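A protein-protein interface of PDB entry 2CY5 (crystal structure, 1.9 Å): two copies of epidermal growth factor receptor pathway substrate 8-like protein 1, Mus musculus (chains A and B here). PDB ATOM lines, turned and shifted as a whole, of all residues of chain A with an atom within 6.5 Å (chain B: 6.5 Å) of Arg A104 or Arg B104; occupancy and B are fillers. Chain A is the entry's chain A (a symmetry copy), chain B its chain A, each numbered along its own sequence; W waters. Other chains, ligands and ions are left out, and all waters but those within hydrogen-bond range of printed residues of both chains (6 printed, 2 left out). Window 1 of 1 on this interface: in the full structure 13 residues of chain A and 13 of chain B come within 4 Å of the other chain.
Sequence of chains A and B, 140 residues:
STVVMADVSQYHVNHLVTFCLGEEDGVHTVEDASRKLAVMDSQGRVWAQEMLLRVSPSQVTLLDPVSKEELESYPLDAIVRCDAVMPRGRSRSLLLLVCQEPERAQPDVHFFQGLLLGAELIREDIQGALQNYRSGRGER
His A15 touches Glu B103, and with the chains exchanged Glu A103 touches His B15. Thr A18 touches Ala B105, and with the chains exchanged Ala A105 touches Thr B18. Cys A20 touches Arg B104, and with the chains exchanged Arg A104 touches Cys B20. Arg A104 touches Asp B108, and with the chains exchanged Asp A108 touches Arg B104. Positions printed for both chains: 15, 17, 18, 19, 20, 74, 100, 101, 102, 103, 104, 105, 106, 107, 108 and 110.
N of Thr B18 is in hydrogen-bond range of O of Glu A103. The backbone NH (N) of Ala A105 lies within hydrogen-bond range of the backbone carbonyl oxygen (O) of Thr B18, at 3.0 Å. SG of Cys B20 is disulfide-bonded to SG of Cys A20. The guanidinium group (NH2) of Arg A104 is in salt-bridge range of the side-chain carboxylate (OE2) of Glu B101, at 3.4 Å. O of Glu B103 sits at hydrogen-bond distance from N of Thr A18 (3.4 Å). NH2 of Arg B104 lies within salt-bridge range of OE2 of Glu A101 (3.4 Å). NH2 of Arg B104 is in salt-bridge range of OD2 of Asp A108 (2.5 Å). N of Ala B105 lies within hydrogen-bond range of O of Thr A18, 3.0 Å away. The side-chain carboxylate (OD2) of Asp B108 is in salt-bridge range of the guanidinium group (NH2) of Arg A104, 2.5 Å away. The guanidinium group (NH1) of Arg B104 sits close to the guanidinium group (NH1) of Arg A104, 3.3 Å away.
Arg A104 touches just these residues of chain B: Thr B18 (3.7 Å), Cys B20 (3.8 Å), Glu B101 (3.4 Å), Arg B104 (3.3 Å) and Asp B108 (2.5 Å). Of the printed residues of chain A, Arg B104 touches Thr A18, Cys A20, Glu A101, Arg A104 and Asp A108. Of the printed residues of chain B, Glu A101 touches Arg B104 (3.4 Å). Printed residues of chain B within 4 Å of His A15: Glu B103. Printed residues of chain A within 4 Å of Asp B108: Arg A104 (2.5 Å). Of the printed residues of chain A, Glu B101 touches Arg A104. The nearest residue of chain B that does not touch Arg A104 is His B110 (4.5 Å). The nearest residue of chain A that does not touch Arg B104 is His A110 (4.5 Å). The nearest printed residue of chain A that does not touch His B15 is Arg A104 (5.4 Å).
A ring nitrogen (NE2) of His B15 is in hydrogen-bond range of the backbone carbonyl oxygen of Val B17. NE2 of His B15 lies within hydrogen-bond range of OG1 of Thr B18, at 2.9 Å. The side-chain amide oxygen (OE1) of Gln B100 lies close to the backbone carbonyl oxygen (O) of Arg B104, at 3.1 Å. The backbone carbonyl oxygen (O) of Val A17 lies within hydrogen-bond range of a ring nitrogen (NE2) of His A15 (3.4 Å). NE2 of His A15 lies within hydrogen-bond range of OG1 of Thr A18 (2.9 Å). The backbone carbonyl oxygen of Arg A104 sits close to the side-chain amide oxygen of Gln A100, 3.1 Å away.
Water W5 lies within hydrogen-bond range of O of Glu A103 (2.5 Å), N of Thr B18 (3.1 Å) and N of Ala A105 (3.2 Å). Water W1 lies within hydrogen-bond range of the backbone carbonyl oxygen of Glu B103 (2.5 Å), the backbone NH of Thr A18 (3.1 Å) and the backbone NH of Ala B105 (3.2 Å). Water W6 lies within hydrogen-bond range of the side-chain amide oxygen of Gln B106 (2.5 Å) and the backbone NH of Cys A20 (3.0 Å). Water W2 bridges OE1 of Gln A106 (2.5 Å) and N of Cys B20 (3.0 Å). Water W4 lies within hydrogen-bond range of the backbone NH (N) of Gln A106 (3.1 Å), the backbone NH (N) of Ala A105 (3.3 Å), the backbone carbonyl oxygen (O) of Thr B18 (3.5 Å) and the side-chain sulfur (SG) of Cys B20 (3.7 Å). Water W3 lies within hydrogen-bond range of the backbone NH (N) of Gln B106 (3.1 Å), the backbone NH (N) of Ala B105 (3.3 Å), the backbone carbonyl oxygen (O) of Thr A18 (3.5 Å) and the side-chain sulfur (SG) of Cys A20 (3.7 Å).
His A15 touches Glu B103 (CE1 to O, 3.3 Å). CA of Arg B104 touches O of Thr A18, 3.7 Å away. NH1 of Arg B104 touches SG of Cys A20, at 3.8 Å. His B15 touches Glu A103 (CE1 to O, 3.3 Å). Arg A104 touches Thr B18 (CA to O, 3.7 Å). Cys B20 touches Arg A104.
Hydrophobic or aromatic side chains of chain B that line the printed part of chain A: His B15 and Ala B105. Printed residues of chain A that touch a printed residue of chain B: His A15, Thr A18, Cys A20, Glu A101, Glu A103, Arg A104, Ala A105 and Asp A108.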
ATOM      1  N   HIS A  15       9.313 -14.895  -5.152  1.00  0.00           N
ATOM      2  CA  HIS A  15       9.226 -14.342  -3.779  1.00  0.00           C
ATOM      3  C   HIS A  15       8.897 -15.506  -2.856  1.00  0.00           C
ATOM      4  O   HIS A  15       8.023 -16.358  -3.201  1.00  0.00           O
ATOM      5  CB  HIS A  15       8.073 -13.315  -3.833  1.00  0.00           C
ATOM      6  CG  HIS A  15       7.686 -12.889  -2.446  1.00  0.00           C
ATOM      7  ND1 HIS A  15       6.651 -13.490  -1.711  1.00  0.00           N
ATOM      8  CD2 HIS A  15       8.241 -11.962  -1.617  1.00  0.00           C
ATOM      9  CE1 HIS A  15       6.603 -12.945  -0.499  1.00  0.00           C
ATOM     10  NE2 HIS A  15       7.551 -12.009  -0.412  1.00  0.00           N
ATOM     11  N   VAL A  17       8.728 -15.202   1.064  1.00  0.00           N
ATOM     12  CA  VAL A  17       7.934 -14.768   2.259  1.00  0.00           C
ATOM     13  C   VAL A  17       8.365 -13.307   2.622  1.00  0.00           C
ATOM     14  O   VAL A  17       9.476 -12.851   2.215  1.00  0.00           O
ATOM     15  CB  VAL A  17       8.361 -15.724   3.508  1.00  0.00           C
ATOM     16  CG1 VAL A  17       9.670 -15.289   4.188  1.00  0.00           C
ATOM     17  CG2 VAL A  17       7.234 -15.609   4.547  1.00  0.00           C
ATOM     18  N   THR A  18       7.450 -12.528   3.227  1.00  0.00           N
ATOM     19  CA  THR A  18       7.739 -11.234   3.777  1.00  0.00           C
ATOM     20  C   THR A  18       7.205 -11.328   5.228  1.00  0.00           C
ATOM     21  O   THR A  18       6.021 -11.809   5.429  1.00  0.00           O
ATOM     22  CB  THR A  18       6.997 -10.225   3.046  1.00  0.00           C
ATOM     23  OG1 THR A  18       7.501 -10.084   1.701  1.00  0.00           O
ATOM     24  CG2 THR A  18       7.122  -8.853   3.802  1.00  0.00           C
ATOM     25  N   PHE A  19       7.952 -10.943   6.239  1.00  0.00           N
ATOM     26  CA  PHE A  19       7.443 -10.980   7.596  1.00  0.00           C
ATOM     27  C   PHE A  19       7.976  -9.786   8.359  1.00  0.00           C
ATOM     28  O   PHE A  19       9.039  -9.237   7.982  1.00  0.00           O
ATOM     29  CB  PHE A  19       7.771 -12.360   8.264  1.00  0.00           C
ATOM     30  CG  PHE A  19       9.251 -12.630   8.508  1.00  0.00           C
ATOM     31  CD1 PHE A  19       9.932 -11.978   9.478  1.00  0.00           C
ATOM     32  CD2 PHE A  19       9.906 -13.592   7.688  1.00  0.00           C
ATOM     33  CE1 PHE A  19      11.343 -12.248   9.692  1.00  0.00           C
ATOM     34  CE2 PHE A  19      11.297 -13.888   7.869  1.00  0.00           C
ATOM     35  CZ  PHE A  19      12.006 -13.229   8.846  1.00  0.00           C
ATOM     36  N   CYS A  20       7.257  -9.315   9.384  1.00  0.00           N
ATOM     37  CA  CYS A  20       7.628  -8.062  10.095  1.00  0.00           C
ATOM     38  C   CYS A  20       8.698  -8.444  11.091  1.00  0.00           C
ATOM     39  O   CYS A  20       8.735  -9.579  11.644  1.00  0.00           O
ATOM     40  CB  CYS A  20       6.358  -7.480  10.966  1.00  0.00           C
ATOM     41  SG  CYS A  20       5.077  -7.382   9.588  1.00  0.00           S
ATOM     42  N   TYR A  74       9.910  -0.193  -3.700  1.00  0.00           N
ATOM     43  CA  TYR A  74      10.620   0.318  -2.566  1.00  0.00           C
ATOM     44  C   TYR A  74      11.687   1.326  -2.969  1.00  0.00           C
ATOM     45  O   TYR A  74      12.726   0.965  -3.535  1.00  0.00           O
ATOM     46  CB  TYR A  74      11.305  -0.843  -1.876  1.00  0.00           C
ATOM     47  CG  TYR A  74      10.426  -2.054  -1.582  1.00  0.00           C
ATOM     48  CD1 TYR A  74      10.350  -3.108  -2.503  1.00  0.00           C
ATOM     49  CD2 TYR A  74       9.632  -2.131  -0.395  1.00  0.00           C
ATOM     50  CE1 TYR A  74       9.523  -4.202  -2.310  1.00  0.00           C
ATOM     51  CE2 TYR A  74       8.791  -3.233  -0.167  1.00  0.00           C
ATOM     52  CZ  TYR A  74       8.733  -4.274  -1.150  1.00  0.00           C
ATOM     53  OH  TYR A  74       7.868  -5.365  -1.074  1.00  0.00           O
ATOM     54  N   GLN A 100      12.190  -0.500   5.475  1.00  0.00           N
ATOM     55  CA  GLN A 100      11.431   0.175   6.610  1.00  0.00           C
ATOM     56  C   GLN A 100      10.565   1.105   5.811  1.00  0.00           C
ATOM     57  O   GLN A 100      11.053   2.140   5.245  1.00  0.00           O
ATOM     58  CB  GLN A 100      12.397   0.993   7.530  1.00  0.00           C
ATOM     59  CG  GLN A 100      11.602   1.905   8.628  1.00  0.00           C
ATOM     60  CD  GLN A 100      10.617   1.000   9.405  1.00  0.00           C
ATOM     61  OE1 GLN A 100       9.404   0.978   9.159  1.00  0.00           O
ATOM     62  NE2 GLN A 100      11.137   0.243  10.299  1.00  0.00           N
ATOM     63  N   GLU A 101       9.344   0.702   5.559  1.00  0.00           N
ATOM     64  CA  GLU A 101       8.423   1.558   4.806  1.00  0.00           C
ATOM     65  C   GLU A 101       8.014   2.724   5.809  1.00  0.00           C
ATOM     66  O   GLU A 101       7.845   2.522   7.089  1.00  0.00           O
ATOM     67  CB  GLU A 101       7.208   0.793   4.405  1.00  0.00           C
ATOM     68  CG  GLU A 101       7.519  -0.257   3.378  1.00  0.00           C
ATOM     69  CD  GLU A 101       6.271  -0.951   2.921  1.00  0.00           C
ATOM     70  OE1 GLU A 101       5.284  -0.240   2.619  1.00  0.00           O
ATOM     71  OE2 GLU A 101       6.251  -2.217   2.852  1.00  0.00           O
ATOM     72  N   PRO A 102       7.916   3.962   5.286  1.00  0.00           N
ATOM     73  CA  PRO A 102       7.552   5.158   6.128  1.00  0.00           C
ATOM     74  C   PRO A 102       6.263   5.029   6.975  1.00  0.00           C
ATOM     75  O   PRO A 102       6.222   5.349   8.178  1.00  0.00           O
ATOM     76  CB  PRO A 102       7.391   6.295   5.080  1.00  0.00           C
ATOM     77  CG  PRO A 102       6.771   5.525   3.822  1.00  0.00           C
ATOM     78  CD  PRO A 102       7.746   4.254   3.829  1.00  0.00           C
ATOM     79  N   GLU A 103       5.288   4.461   6.372  1.00  0.00           N
ATOM     80  CA  GLU A 103       4.039   4.236   7.056  1.00  0.00           C
ATOM     81  C   GLU A 103       3.914   3.104   8.101  1.00  0.00           C
ATOM     82  O   GLU A 103       2.903   2.990   8.905  1.00  0.00           O
ATOM     83  CB  GLU A 103       3.025   3.951   6.013  1.00  0.00           C
ATOM     84  CG  GLU A 103       2.559   5.204   5.320  1.00  0.00           C
ATOM     85  CD  GLU A 103       3.658   5.985   4.662  1.00  0.00           C
ATOM     86  OE1 GLU A 103       4.437   6.608   5.416  1.00  0.00           O
ATOM     87  OE2 GLU A 103       3.738   5.983   3.405  1.00  0.00           O
ATOM     88  N   ARG A 104       4.865   2.182   8.041  1.00  0.00           N
ATOM     89  CA  ARG A 104       4.796   1.021   8.944  1.00  0.00           C
ATOM     90  C   ARG A 104       5.526   1.225  10.222  1.00  0.00           C
ATOM     91  O   ARG A 104       6.584   1.801  10.248  1.00  0.00           O
ATOM     92  CB  ARG A 104       5.359  -0.281   8.196  1.00  0.00           C
ATOM     93  CG  ARG A 104       4.342  -0.613   7.033  1.00  0.00           C
ATOM     94  CD  ARG A 104       4.828  -1.925   6.344  1.00  0.00           C
ATOM     95  NE  ARG A 104       3.695  -2.399   5.690  1.00  0.00           N
ATOM     96  CZ  ARG A 104       2.882  -3.334   6.183  1.00  0.00           C
ATOM     97  NH1 ARG A 104       3.078  -3.921   7.320  1.00  0.00           N
ATOM     98  NH2 ARG A 104       1.901  -3.696   5.468  1.00  0.00           N
ATOM     99  N   ALA A 105       5.038   0.631  11.269  1.00  0.00           N
ATOM    100  CA  ALA A 105       5.667   0.799  12.595  1.00  0.00           C
ATOM    101  C   ALA A 105       6.987  -0.049  12.708  1.00  0.00           C
ATOM    102  O   ALA A 105       7.880   0.307  13.489  1.00  0.00           O
ATOM    103  CB  ALA A 105       4.748   0.318  13.622  1.00  0.00           C
ATOM    104  N   GLN A 106       7.132  -1.112  11.896  1.00  0.00           N
ATOM    105  CA  GLN A 106       8.282  -2.007  12.018  1.00  0.00           C
ATOM    106  C   GLN A 106       8.857  -2.277  10.633  1.00  0.00           C
ATOM    107  O   GLN A 106       8.136  -2.183   9.633  1.00  0.00           O
ATOM    108  CB  GLN A 106       7.821  -3.310  12.588  1.00  0.00           C
ATOM    109  CG  GLN A 106       7.525  -3.220  14.159  1.00  0.00           C
ATOM    110  CD  GLN A 106       6.903  -4.501  14.768  1.00  0.00           C
ATOM    111  OE1 GLN A 106       6.341  -5.416  14.038  1.00  0.00           O
ATOM    112  NE2 GLN A 106       6.951  -4.564  16.146  1.00  0.00           N
ATOM    113  N   PRO A 107      10.143  -2.659  10.587  1.00  0.00           N
ATOM    114  CA  PRO A 107      10.747  -2.969   9.262  1.00  0.00           C
ATOM    115  C   PRO A 107      10.228  -4.397   8.870  1.00  0.00           C
ATOM    116  O   PRO A 107       9.696  -5.159   9.696  1.00  0.00           O
ATOM    117  CB  PRO A 107      12.223  -3.143   9.537  1.00  0.00           C
ATOM    118  CG  PRO A 107      12.379  -2.996  11.088  1.00  0.00           C
ATOM    119  CD  PRO A 107      11.136  -2.570  11.682  1.00  0.00           C
ATOM    120  N   ASP A 108      10.422  -4.760   7.589  1.00  0.00           N
ATOM    121  CA  ASP A 108       9.985  -6.096   7.148  1.00  0.00           C
ATOM    122  C   ASP A 108      11.242  -6.767   6.515  1.00  0.00           C
ATOM    123  O   ASP A 108      12.109  -6.018   5.910  1.00  0.00           O
ATOM    124  CB  ASP A 108       9.043  -5.907   5.961  1.00  0.00           C
ATOM    125  CG  ASP A 108       7.723  -5.201   6.334  1.00  0.00           C
ATOM    126  OD1 ASP A 108       7.249  -5.728   7.357  1.00  0.00           O
ATOM    127  OD2 ASP A 108       7.204  -4.240   5.640  1.00  0.00           O
ATOM    128  N   HIS A 110      12.122  -9.350   3.500  1.00  0.00           N
ATOM    129  CA  HIS A 110      11.565 -10.007   2.317  1.00  0.00           C
ATOM    130  C   HIS A 110      12.665 -11.085   1.815  1.00  0.00           C
ATOM    131  O   HIS A 110      13.889 -10.763   1.700  1.00  0.00           O
ATOM    132  CB  HIS A 110      11.390  -9.031   1.214  1.00  0.00           C
ATOM    133  CG  HIS A 110      10.518  -7.840   1.532  1.00  0.00           C
ATOM    134  ND1 HIS A 110       9.142  -7.881   1.395  1.00  0.00           N
ATOM    135  CD2 HIS A 110      10.821  -6.590   2.006  1.00  0.00           C
ATOM    136  CE1 HIS A 110       8.643  -6.709   1.799  1.00  0.00           C
ATOM    137  NE2 HIS A 110       9.630  -5.918   2.182  1.00  0.00           N
ATOM    138  N   HIS B  15      -3.283   9.319   7.810  1.00  0.00           N
ATOM    139  CA  HIS B  15      -2.920   7.946   8.237  1.00  0.00           C
ATOM    140  C   HIS B  15      -2.241   8.072   9.593  1.00  0.00           C
ATOM    141  O   HIS B  15      -1.389   8.992   9.790  1.00  0.00           O
ATOM    142  CB  HIS B  15      -1.941   7.436   7.156  1.00  0.00           C
ATOM    143  CG  HIS B  15      -1.271   6.172   7.611  1.00  0.00           C
ATOM    144  ND1 HIS B  15      -0.024   6.143   8.256  1.00  0.00           N
ATOM    145  CD2 HIS B  15      -1.703   4.881   7.581  1.00  0.00           C
ATOM    146  CE1 HIS B  15       0.263   4.891   8.598  1.00  0.00           C
ATOM    147  NE2 HIS B  15      -0.733   4.099   8.196  1.00  0.00           N
ATOM    148  N   VAL B  17      -1.135   4.989  11.774  1.00  0.00           N
ATOM    149  CA  VAL B  17      -0.123   3.908  12.002  1.00  0.00           C
ATOM    150  C   VAL B  17      -0.612   2.622  11.255  1.00  0.00           C
ATOM    151  O   VAL B  17      -1.834   2.494  10.940  1.00  0.00           O
ATOM    152  CB  VAL B  17      -0.113   3.569  13.596  1.00  0.00           C
ATOM    153  CG1 VAL B  17      -1.252   2.628  14.026  1.00  0.00           C
ATOM    154  CG2 VAL B  17       1.217   2.852  13.878  1.00  0.00           C
ATOM    155  N   THR B  18       0.330   1.761  10.828  1.00  0.00           N
ATOM    156  CA  THR B  18       0.041   0.463  10.286  1.00  0.00           C
ATOM    157  C   THR B  18       0.928  -0.487  11.129  1.00  0.00           C
ATOM    158  O   THR B  18       2.172  -0.183  11.316  1.00  0.00           O
ATOM    159  CB  THR B  18       0.459   0.420   8.898  1.00  0.00           C
ATOM    160  OG1 THR B  18      -0.377   1.264   8.079  1.00  0.00           O
ATOM    161  CG2 THR B  18       0.372  -1.063   8.386  1.00  0.00           C
ATOM    162  N   PHE B  19       0.418  -1.576  11.663  1.00  0.00           N
ATOM    163  CA  PHE B  19       1.251  -2.497  12.410  1.00  0.00           C
ATOM    164  C   PHE B  19       0.792  -3.914  12.136  1.00  0.00           C
ATOM    165  O   PHE B  19      -0.386  -4.120  11.759  1.00  0.00           O
ATOM    166  CB  PHE B  19       1.258  -2.114  13.930  1.00  0.00           C
ATOM    167  CG  PHE B  19      -0.074  -2.284  14.652  1.00  0.00           C
ATOM    168  CD1 PHE B  19      -0.560  -3.511  14.945  1.00  0.00           C
ATOM    169  CD2 PHE B  19      -0.799  -1.114  15.014  1.00  0.00           C
ATOM    170  CE1 PHE B  19      -1.834  -3.651  15.631  1.00  0.00           C
ATOM    171  CE2 PHE B  19      -2.058  -1.209  15.693  1.00  0.00           C
ATOM    172  CZ  PHE B  19      -2.571  -2.450  15.994  1.00  0.00           C
ATOM    173  N   CYS B  20       1.686  -4.903  12.249  1.00  0.00           N
ATOM    174  CA  CYS B  20       1.364  -6.301  11.858  1.00  0.00           C
ATOM    175  C   CYS B  20       0.627  -6.907  13.030  1.00  0.00           C
ATOM    176  O   CYS B  20       0.858  -6.568  14.224  1.00  0.00           O
ATOM    177  CB  CYS B  20       2.737  -7.188  11.655  1.00  0.00           C
ATOM    178  SG  CYS B  20       3.613  -6.088  10.402  1.00  0.00           S
ATOM    179  N   TYR B  74      -5.164  -1.569  -2.013  1.00  0.00           N
ATOM    180  CA  TYR B  74      -5.622  -2.829  -1.506  1.00  0.00           C
ATOM    181  C   TYR B  74      -6.864  -3.320  -2.238  1.00  0.00           C
ATOM    182  O   TYR B  74      -7.963  -2.780  -2.065  1.00  0.00           O
ATOM    183  CB  TYR B  74      -5.977  -2.647  -0.045  1.00  0.00           C
ATOM    184  CG  TYR B  74      -4.921  -1.962   0.816  1.00  0.00           C
ATOM    185  CD1 TYR B  74      -4.958  -0.573   1.002  1.00  0.00           C
ATOM    186  CD2 TYR B  74      -3.853  -2.699   1.416  1.00  0.00           C
ATOM    187  CE1 TYR B  74      -3.991   0.104   1.725  1.00  0.00           C
ATOM    188  CE2 TYR B  74      -2.862  -2.042   2.164  1.00  0.00           C
ATOM    189  CZ  TYR B  74      -2.933  -0.618   2.306  1.00  0.00           C
ATOM    190  OH  TYR B  74      -1.958   0.148   2.945  1.00  0.00           O
ATOM    191  N   GLN B 100      -5.034  -8.415   4.514  1.00  0.00           N
ATOM    192  CA  GLN B 100      -4.098  -9.616   4.534  1.00  0.00           C
ATOM    193  C   GLN B 100      -3.570  -9.543   3.131  1.00  0.00           C
ATOM    194  O   GLN B 100      -4.298  -9.866   2.133  1.00  0.00           O
ATOM    195  CB  GLN B 100      -4.890 -10.949   4.744  1.00  0.00           C
ATOM    196  CG  GLN B 100      -3.956 -12.276   4.557  1.00  0.00           C
ATOM    197  CD  GLN B 100      -2.712 -12.139   5.467  1.00  0.00           C
ATOM    198  OE1 GLN B 100      -1.604 -11.804   5.026  1.00  0.00           O
ATOM    199  NE2 GLN B 100      -2.903 -12.357   6.715  1.00  0.00           N
ATOM    200  N   GLU B 101      -2.413  -8.950   2.968  1.00  0.00           N
ATOM    201  CA  GLU B 101      -1.812  -8.856   1.634  1.00  0.00           C
ATOM    202  C   GLU B 101      -1.301 -10.325   1.296  1.00  0.00           C
ATOM    203  O   GLU B 101      -0.797 -11.119   2.202  1.00  0.00           O
ATOM    204  CB  GLU B 101      -0.657  -7.915   1.646  1.00  0.00           C
ATOM    205  CG  GLU B 101      -1.093  -6.493   1.859  1.00  0.00           C
ATOM    206  CD  GLU B 101       0.072  -5.554   1.776  1.00  0.00           C
ATOM    207  OE1 GLU B 101       0.866  -5.689   0.815  1.00  0.00           O
ATOM    208  OE2 GLU B 101       0.218  -4.661   2.665  1.00  0.00           O
ATOM    209  N   PRO B 102      -1.478 -10.748   0.028  1.00  0.00           N
ATOM    210  CA  PRO B 102      -1.054 -12.122  -0.422  1.00  0.00           C
ATOM    211  C   PRO B 102       0.412 -12.517  -0.119  1.00  0.00           C
ATOM    212  O   PRO B 102       0.715 -13.615   0.386  1.00  0.00           O
ATOM    213  CB  PRO B 102      -1.290 -12.082  -1.957  1.00  0.00           C
ATOM    214  CG  PRO B 102      -0.920 -10.570  -2.329  1.00  0.00           C
ATOM    215  CD  PRO B 102      -1.711  -9.844  -1.141  1.00  0.00           C
ATOM    216  N   GLU B 103       1.264 -11.584  -0.318  1.00  0.00           N
ATOM    217  CA  GLU B 103       2.661 -11.798  -0.036  1.00  0.00           C
ATOM    218  C   GLU B 103       3.171 -11.807   1.424  1.00  0.00           C
ATOM    219  O   GLU B 103       4.356 -12.211   1.758  1.00  0.00           O
ATOM    220  CB  GLU B 103       3.409 -10.723  -0.729  1.00  0.00           C
ATOM    221  CG  GLU B 103       3.541 -10.988  -2.206  1.00  0.00           C
ATOM    222  CD  GLU B 103       2.232 -11.143  -2.920  1.00  0.00           C
ATOM    223  OE1 GLU B 103       1.599 -12.203  -2.716  1.00  0.00           O
ATOM    224  OE2 GLU B 103       1.842 -10.221  -3.684  1.00  0.00           O
ATOM    225  N   ARG B 104       2.345 -11.260   2.306  1.00  0.00           N
ATOM    226  CA  ARG B 104       2.769 -11.150   3.711  1.00  0.00           C
ATOM    227  C   ARG B 104       2.363 -12.314   4.541  1.00  0.00           C
ATOM    228  O   ARG B 104       1.286 -12.835   4.395  1.00  0.00           O
ATOM    229  CB  ARG B 104       2.189  -9.798   4.348  1.00  0.00           C
ATOM    230  CG  ARG B 104       2.914  -8.602   3.614  1.00  0.00           C
ATOM    231  CD  ARG B 104       2.424  -7.277   4.276  1.00  0.00           C
ATOM    232  NE  ARG B 104       3.405  -6.350   3.935  1.00  0.00           N
ATOM    233  CZ  ARG B 104       4.416  -6.003   4.732  1.00  0.00           C
ATOM    234  NH1 ARG B 104       4.578  -6.477   5.926  1.00  0.00           N
ATOM    235  NH2 ARG B 104       5.222  -5.122   4.308  1.00  0.00           N
ATOM    236  N   ALA B 105       3.161 -12.640   5.512  1.00  0.00           N
ATOM    237  CA  ALA B 105       2.867 -13.804   6.374  1.00  0.00           C
ATOM    238  C   ALA B 105       1.722 -13.475   7.401  1.00  0.00           C
ATOM    239  O   ALA B 105       1.018 -14.391   7.848  1.00  0.00           O
ATOM    240  CB  ALA B 105       4.061 -14.141   7.142  1.00  0.00           C
ATOM    241  N   GLN B 106       1.501 -12.186   7.717  1.00  0.00           N
ATOM    242  CA  GLN B 106       0.527 -11.813   8.742  1.00  0.00           C
ATOM    243  C   GLN B 106      -0.341 -10.675   8.220  1.00  0.00           C
ATOM    244  O   GLN B 106       0.093  -9.915   7.346  1.00  0.00           O
ATOM    245  CB  GLN B 106       1.260 -11.319   9.947  1.00  0.00           C
ATOM    246  CG  GLN B 106       1.927 -12.508  10.788  1.00  0.00           C
ATOM    247  CD  GLN B 106       2.822 -12.038  11.962  1.00  0.00           C
ATOM    248  OE1 GLN B 106       3.285 -10.828  12.042  1.00  0.00           O
ATOM    249  NE2 GLN B 106       3.127 -13.022  12.880  1.00  0.00           N
ATOM    250  N   PRO B 107      -1.546 -10.534   8.795  1.00  0.00           N
ATOM    251  CA  PRO B 107      -2.422  -9.416   8.346  1.00  0.00           C
ATOM    252  C   PRO B 107      -1.858  -8.120   9.029  1.00  0.00           C
ATOM    253  O   PRO B 107      -1.054  -8.166   9.976  1.00  0.00           O
ATOM    254  CB  PRO B 107      -3.753  -9.672   9.016  1.00  0.00           C
ATOM    255  CG  PRO B 107      -3.533 -10.935   9.915  1.00  0.00           C
ATOM    256  CD  PRO B 107      -2.238 -11.516   9.661  1.00  0.00           C
ATOM    257  N   ASP B 108      -2.323  -6.955   8.546  1.00  0.00           N
ATOM    258  CA  ASP B 108      -1.861  -5.692   9.150  1.00  0.00           C
ATOM    259  C   ASP B 108      -3.151  -4.921   9.565  1.00  0.00           C
ATOM    260  O   ASP B 108      -4.222  -5.069   8.849  1.00  0.00           O
ATOM    261  CB  ASP B 108      -1.272  -4.832   8.034  1.00  0.00           C
ATOM    262  CG  ASP B 108       0.010  -5.427   7.415  1.00  0.00           C
ATOM    263  OD1 ASP B 108       0.781  -5.781   8.326  1.00  0.00           O
ATOM    264  OD2 ASP B 108       0.226  -5.491   6.141  1.00  0.00           O
ATOM    265  N   HIS B 110      -4.456  -1.079   9.812  1.00  0.00           N
ATOM    266  CA  HIS B 110      -4.141   0.296   9.420  1.00  0.00           C
ATOM    267  C   HIS B 110      -5.201   1.257  10.178  1.00  0.00           C
ATOM    268  O   HIS B 110      -6.444   0.990  10.174  1.00  0.00           O
ATOM    269  CB  HIS B 110      -4.358   0.485   7.965  1.00  0.00           C
ATOM    270  CG  HIS B 110      -3.576  -0.441   7.065  1.00  0.00           C
ATOM    271  ND1 HIS B 110      -2.282  -0.156   6.667  1.00  0.00           N
ATOM    272  CD2 HIS B 110      -3.891  -1.655   6.512  1.00  0.00           C
ATOM    273  CE1 HIS B 110      -1.834  -1.175   5.928  1.00  0.00           C
ATOM    274  NE2 HIS B 110      -2.778  -2.095   5.827  1.00  0.00           N
HETATM  275  O   HOH W   1       4.847 -14.192   3.265  1.00  0.00           O
HETATM  276  O   HOH W   2       4.330  -3.996  13.379  1.00  0.00           O
HETATM  277  O   HOH W   3       3.829 -10.207   7.608  1.00  0.00           O
HETATM  278  O   HOH W   4       4.641  -2.608  10.945  1.00  0.00           O
HETATM  279  O   HOH W   5       3.032   3.132  11.434  1.00  0.00           O
HETATM  280  O   HOH W   6       4.893 -11.053  10.079  1.00  0.00           O
